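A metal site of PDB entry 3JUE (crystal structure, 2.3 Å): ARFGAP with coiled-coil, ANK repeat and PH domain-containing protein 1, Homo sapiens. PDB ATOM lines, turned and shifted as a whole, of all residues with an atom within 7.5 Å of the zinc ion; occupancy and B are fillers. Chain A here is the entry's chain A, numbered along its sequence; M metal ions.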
ATOM      1  N   GLN A  47      -4.855 -17.113   7.387  1.00  0.00           N
ATOM      2  CA  GLN A  47      -4.868 -18.581   7.456  1.00  0.00           C
ATOM      3  C   GLN A  47      -3.816 -19.007   8.497  1.00  0.00           C
ATOM      4  O   GLN A  47      -2.712 -18.461   8.521  1.00  0.00           O
ATOM      5  CB  GLN A  47      -4.492 -19.209   6.107  1.00  0.00           C
ATOM      6  CG  GLN A  47      -5.575 -19.165   5.014  1.00  0.00           C
ATOM      7  CD  GLN A  47      -5.761 -17.779   4.444  1.00  0.00           C
ATOM      8  OE1 GLN A  47      -4.789 -17.113   4.096  1.00  0.00           O
ATOM      9  NE2 GLN A  47      -7.012 -17.316   4.361  1.00  0.00           N
ATOM     10  N   CYS A  48      -4.144 -19.984   9.334  1.00  0.00           N
ATOM     11  CA  CYS A  48      -3.163 -20.528  10.283  1.00  0.00           C
ATOM     12  C   CYS A  48      -1.892 -20.935   9.541  1.00  0.00           C
ATOM     13  O   CYS A  48      -1.975 -21.519   8.452  1.00  0.00           O
ATOM     14  CB  CYS A  48      -3.710 -21.754  11.022  1.00  0.00           C
ATOM     15  SG  CYS A  48      -2.441 -22.587  12.004  1.00  0.00           S
ATOM     16  N   CYS A  49      -0.731 -20.645  10.147  1.00  0.00           N
ATOM     17  CA  CYS A  49       0.567 -20.915   9.501  1.00  0.00           C
ATOM     18  C   CYS A  49       0.773 -22.409   9.233  1.00  0.00           C
ATOM     19  O   CYS A  49       1.323 -22.812   8.188  1.00  0.00           O
ATOM     20  CB  CYS A  49       1.708 -20.392  10.390  1.00  0.00           C
ATOM     21  SG  CYS A  49       3.348 -20.357   9.560  1.00  0.00           S
ATOM     22  N   ASP A  50       0.297 -23.243  10.157  1.00  0.00           N
ATOM     23  CA  ASP A  50       0.604 -24.655  10.059  1.00  0.00           C
ATOM     24  C   ASP A  50      -0.474 -25.522   9.383  1.00  0.00           C
ATOM     25  O   ASP A  50      -0.145 -26.576   8.832  1.00  0.00           O
ATOM     26  CB  ASP A  50       1.011 -25.189  11.425  1.00  0.00           C
ATOM     27  CG  ASP A  50       2.201 -24.432  12.017  1.00  0.00           C
ATOM     28  OD1 ASP A  50       3.050 -23.906  11.253  1.00  0.00           O
ATOM     29  OD2 ASP A  50       2.314 -24.393  13.264  1.00  0.00           O
ATOM     30  N   CYS A  51      -1.730 -25.062   9.381  1.00  0.00           N
ATOM     31  CA  CYS A  51      -2.851 -25.871   8.855  1.00  0.00           C
ATOM     32  C   CYS A  51      -3.895 -25.088   8.039  1.00  0.00           C
ATOM     33  O   CYS A  51      -4.867 -25.676   7.601  1.00  0.00           O
ATOM     34  CB  CYS A  51      -3.567 -26.612   9.974  1.00  0.00           C
ATOM     35  SG  CYS A  51      -4.770 -25.603  10.860  1.00  0.00           S
ATOM     36  N   ARG A  52      -3.683 -23.787   7.864  1.00  0.00           N
ATOM     37  CA  ARG A  52      -4.542 -22.903   7.049  1.00  0.00           C
ATOM     38  C   ARG A  52      -5.953 -22.720   7.585  1.00  0.00           C
ATOM     39  O   ARG A  52      -6.830 -22.250   6.852  1.00  0.00           O
ATOM     40  CB  ARG A  52      -4.569 -23.321   5.560  1.00  0.00           C
ATOM     41  CG  ARG A  52      -3.178 -23.378   4.956  1.00  0.00           C
ATOM     42  CD  ARG A  52      -3.175 -23.742   3.492  1.00  0.00           C
ATOM     43  NE  ARG A  52      -3.853 -22.734   2.698  1.00  0.00           N
ATOM     44  CZ  ARG A  52      -3.364 -21.533   2.399  1.00  0.00           C
ATOM     45  NH1 ARG A  52      -2.154 -21.176   2.831  1.00  0.00           N
ATOM     46  NH2 ARG A  52      -4.075 -20.679   1.678  1.00  0.00           N
ATOM     47  N   GLU A  53      -6.169 -23.089   8.844  1.00  0.00           N
ATOM     48  CA  GLU A  53      -7.403 -22.781   9.528  1.00  0.00           C
ATOM     49  C   GLU A  53      -7.614 -21.261   9.442  1.00  0.00           C
ATOM     50  O   GLU A  53      -6.703 -20.490   9.700  1.00  0.00           O
ATOM     51  CB  GLU A  53      -7.327 -23.235  11.002  1.00  0.00           C
ATOM     52  CG  GLU A  53      -8.506 -22.771  11.889  1.00  0.00           C
ATOM     53  CD  GLU A  53      -9.716 -23.668  11.767  1.00  0.00           C
ATOM     54  OE1 GLU A  53      -9.527 -24.908  11.683  1.00  0.00           O
ATOM     55  OE2 GLU A  53     -10.859 -23.145  11.776  1.00  0.00           O
ATOM     56  N   PRO A  54      -8.821 -20.835   9.030  1.00  0.00           N
ATOM     57  CA  PRO A  54      -9.085 -19.402   8.875  1.00  0.00           C
ATOM     58  C   PRO A  54      -9.188 -18.659  10.199  1.00  0.00           C
ATOM     59  O   PRO A  54      -9.570 -19.238  11.199  1.00  0.00           O
ATOM     60  CB  PRO A  54     -10.444 -19.361   8.148  1.00  0.00           C
ATOM     61  CG  PRO A  54     -10.866 -20.753   7.916  1.00  0.00           C
ATOM     62  CD  PRO A  54      -9.901 -21.704   8.514  1.00  0.00           C
ATOM     63  N   PRO A  56      -6.926 -17.184  12.385  1.00  0.00           N
ATOM     64  CA  PRO A  56      -6.153 -17.573  13.566  1.00  0.00           C
ATOM     65  C   PRO A  56      -6.046 -16.397  14.555  1.00  0.00           C
ATOM     66  O   PRO A  56      -5.770 -15.267  14.140  1.00  0.00           O
ATOM     67  CB  PRO A  56      -4.780 -17.915  12.979  1.00  0.00           C
ATOM     68  CG  PRO A  56      -4.677 -17.033  11.786  1.00  0.00           C
ATOM     69  CD  PRO A  56      -6.062 -16.950  11.209  1.00  0.00           C
ATOM     70  N   THR A  66       1.015 -16.320  12.855  1.00  0.00           N
ATOM     71  CA  THR A  66      -0.318 -16.556  13.449  1.00  0.00           C
ATOM     72  C   THR A  66      -0.746 -18.026  13.368  1.00  0.00           C
ATOM     73  O   THR A  66      -0.432 -18.755  12.418  1.00  0.00           O
ATOM     74  CB  THR A  66      -1.384 -15.716  12.775  1.00  0.00           C
ATOM     75  OG1 THR A  66      -1.429 -16.062  11.395  1.00  0.00           O
ATOM     76  CG2 THR A  66      -1.100 -14.229  12.928  1.00  0.00           C
ATOM     77  N   LEU A  67      -1.483 -18.452  14.395  1.00  0.00           N
ATOM     78  CA  LEU A  67      -1.814 -19.840  14.611  1.00  0.00           C
ATOM     79  C   LEU A  67      -3.232 -19.922  15.154  1.00  0.00           C
ATOM     80  O   LEU A  67      -3.710 -18.985  15.819  1.00  0.00           O
ATOM     81  CB  LEU A  67      -0.859 -20.470  15.639  1.00  0.00           C
ATOM     82  CG  LEU A  67       0.620 -20.308  15.319  1.00  0.00           C
ATOM     83  CD1 LEU A  67       1.468 -20.550  16.577  1.00  0.00           C
ATOM     84  CD2 LEU A  67       1.066 -21.234  14.159  1.00  0.00           C
ATOM     85  N   CYS A  68      -3.906 -21.046  14.831  1.00  0.00           N
ATOM     86  CA  CYS A  68      -5.225 -21.336  15.323  1.00  0.00           C
ATOM     87  C   CYS A  68      -5.114 -21.926  16.719  1.00  0.00           C
ATOM     88  O   CYS A  68      -3.997 -22.120  17.239  1.00  0.00           O
ATOM     89  CB  CYS A  68      -5.936 -22.312  14.366  1.00  0.00           C
ATOM     90  SG  CYS A  68      -5.273 -24.022  14.290  1.00  0.00           S
ATOM     91  N   ILE A  69      -6.266 -22.202  17.321  1.00  0.00           N
ATOM     92  CA  ILE A  69      -6.352 -22.742  18.674  1.00  0.00           C
ATOM     93  C   ILE A  69      -5.546 -24.037  18.755  1.00  0.00           C
ATOM     94  O   ILE A  69      -4.652 -24.178  19.600  1.00  0.00           O
ATOM     95  CB  ILE A  69      -7.835 -23.028  19.095  1.00  0.00           C
ATOM     96  CG1 ILE A  69      -8.689 -21.750  19.020  1.00  0.00           C
ATOM     97  CG2 ILE A  69      -7.908 -23.663  20.495  1.00  0.00           C
ATOM     98  CD1 ILE A  69     -10.137 -21.898  19.591  1.00  0.00           C
ATOM     99  N   GLN A  70      -5.872 -24.964  17.850  1.00  0.00           N
ATOM    100  CA  GLN A  70      -5.236 -26.286  17.797  1.00  0.00           C
ATOM    101  C   GLN A  70      -3.714 -26.209  17.627  1.00  0.00           C
ATOM    102  O   GLN A  70      -2.972 -26.769  18.420  1.00  0.00           O
ATOM    103  CB  GLN A  70      -5.870 -27.122  16.673  1.00  0.00           C
ATOM    104  CG  GLN A  70      -5.586 -28.602  16.794  1.00  0.00           C
ATOM    105  CD  GLN A  70      -6.531 -29.469  16.000  1.00  0.00           C
ATOM    106  OE1 GLN A  70      -6.907 -29.139  14.868  1.00  0.00           O
ATOM    107  NE2 GLN A  70      -6.904 -30.595  16.574  1.00  0.00           N
ATOM    108  N   CYS A  71      -3.238 -25.516  16.582  1.00  0.00           N
ATOM    109  CA  CYS A  71      -1.795 -25.430  16.361  1.00  0.00           C
ATOM    110  C   CYS A  71      -1.021 -24.641  17.428  1.00  0.00           C
ATOM    111  O   CYS A  71       0.140 -24.981  17.715  1.00  0.00           O
ATOM    112  CB  CYS A  71      -1.475 -24.912  14.960  1.00  0.00           C
ATOM    113  SG  CYS A  71      -2.037 -26.045  13.660  1.00  0.00           S
ATOM    114  N   SER A  72      -1.626 -23.590  18.003  1.00  0.00           N
ATOM    115  CA  SER A  72      -0.933 -22.849  19.072  1.00  0.00           C
ATOM    116  C   SER A  72      -0.749 -23.730  20.304  1.00  0.00           C
ATOM    117  O   SER A  72       0.285 -23.643  20.979  1.00  0.00           O
ATOM    118  CB  SER A  72      -1.679 -21.560  19.440  1.00  0.00           C
ATOM    119  OG  SER A  72      -3.020 -21.832  19.823  1.00  0.00           O
ATOM    120  N   ILE A  74      -0.348 -26.957  20.238  1.00  0.00           N
ATOM    121  CA  ILE A  74       0.810 -27.794  19.891  1.00  0.00           C
ATOM    122  C   ILE A  74       2.134 -27.031  20.036  1.00  0.00           C
ATOM    123  O   ILE A  74       3.073 -27.545  20.625  1.00  0.00           O
ATOM    124  CB  ILE A  74       0.673 -28.437  18.456  1.00  0.00           C
ATOM    125  CG1 ILE A  74      -0.550 -29.380  18.406  1.00  0.00           C
ATOM    126  CG2 ILE A  74       1.932 -29.227  18.098  1.00  0.00           C
ATOM    127  CD1 ILE A  74      -1.084 -29.671  17.007  1.00  0.00           C
ATOM    128  N   PRO A 125      -1.002 -30.377   6.469  1.00  0.00           N
ATOM    129  CA  PRO A 125      -2.353 -30.582   6.978  1.00  0.00           C
ATOM    130  C   PRO A 125      -3.292 -29.439   6.607  1.00  0.00           C
ATOM    131  O   PRO A 125      -2.847 -28.290   6.450  1.00  0.00           O
ATOM    132  CB  PRO A 125      -2.151 -30.604   8.509  1.00  0.00           C
ATOM    133  CG  PRO A 125      -0.681 -30.532   8.760  1.00  0.00           C
ATOM    134  CD  PRO A 125      -0.086 -29.938   7.529  1.00  0.00           C
ATOM    135  N   GLY A 126      -4.581 -29.756   6.473  1.00  0.00           N
ATOM    136  CA  GLY A 126      -5.634 -28.749   6.365  1.00  0.00           C
ATOM    137  C   GLY A 126      -6.351 -28.570   7.708  1.00  0.00           C
ATOM    138  O   GLY A 126      -6.079 -29.293   8.659  1.00  0.00           O
ATOM    139  N   PRO A 127      -7.295 -27.612   7.763  1.00  0.00           N
ATOM    140  CA  PRO A 127      -7.964 -27.262   9.030  1.00  0.00           C
ATOM    141  C   PRO A 127      -8.595 -28.440   9.755  1.00  0.00           C
ATOM    142  O   PRO A 127      -8.577 -28.479  10.989  1.00  0.00           O
ATOM    143  CB  PRO A 127      -9.043 -26.260   8.602  1.00  0.00           C
ATOM    144  CG  PRO A 127      -8.566 -25.715   7.297  1.00  0.00           C
ATOM    145  CD  PRO A 127      -7.826 -26.831   6.629  1.00  0.00           C
ATOM    146  N   LYS A 134      -1.389 -32.855  12.698  1.00  0.00           N
ATOM    147  CA  LYS A 134      -0.834 -31.510  12.924  1.00  0.00           C
ATOM    148  C   LYS A 134       0.428 -31.547  13.810  1.00  0.00           C
ATOM    149  O   LYS A 134       1.404 -30.869  13.488  1.00  0.00           O
ATOM    150  CB  LYS A 134      -1.908 -30.546  13.452  1.00  0.00           C
ATOM    151  CG  LYS A 134      -3.042 -30.297  12.477  1.00  0.00           C
ATOM    152  CD  LYS A 134      -4.089 -29.336  12.980  1.00  0.00           C
ATOM    153  CE  LYS A 134      -5.232 -29.245  11.974  1.00  0.00           C
ATOM    154  NZ  LYS A 134      -6.233 -28.182  12.269  1.00  0.00           N
ATOM    155  N   ILE A 138       4.005 -30.108  12.663  1.00  0.00           N
ATOM    156  CA  ILE A 138       4.622 -29.029  13.444  1.00  0.00           C
ATOM    157  C   ILE A 138       6.014 -29.432  13.958  1.00  0.00           C
ATOM    158  O   ILE A 138       6.957 -28.679  13.809  1.00  0.00           O
ATOM    159  CB  ILE A 138       3.657 -28.494  14.548  1.00  0.00           C
ATOM    160  CG1 ILE A 138       2.476 -27.780  13.878  1.00  0.00           C
ATOM    161  CG2 ILE A 138       4.354 -27.502  15.483  1.00  0.00           C
ATOM    162  CD1 ILE A 138       1.326 -27.466  14.788  1.00  0.00           C
HETATM  163 ZN    ZN M   1      -3.599 -24.584  12.666  1.00  0.00          ZN
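The side-chain sulfur of Cys 51 sits close to the backbone NH of Glu 53 (3.5 Å).
The side-chain sulfur (SG) of Cys 51 sits close to the side-chain amino group (NZ) of Lys 134 (3.3 Å).
The side-chain sulfur (SG) of Cys 68 sits close to the backbone NH (N) of Gln 70.
O of Cys 68 is in hydrogen-bond range of OG of Ser 72, at 2.8 Å.
N of Cys 48 lies within hydrogen-bond range of O of Glu 53 (2.6 Å).
The side-chain sulfur (SG) of Cys 48 sits close to the backbone NH (N) of Asp 50 (3.4 Å).
The side-chain sulfur (SG) of Cys 71 binds the zinc ion, at 2.4 Å.
SG of Cys 51 binds the zinc ion, at 2.4 Å.
The zinc ion is bound by SG of Cys 68.
SG of Cys 48 binds the zinc ion.
The zinc ion has four donor atoms within binding distance.
Within 4 Å of the zinc ion: Cys 48, Cys 51, Cys 68 and Cys 71.
Along chain A the residues within 4 Å of the zinc ion span positions 48 to 71.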
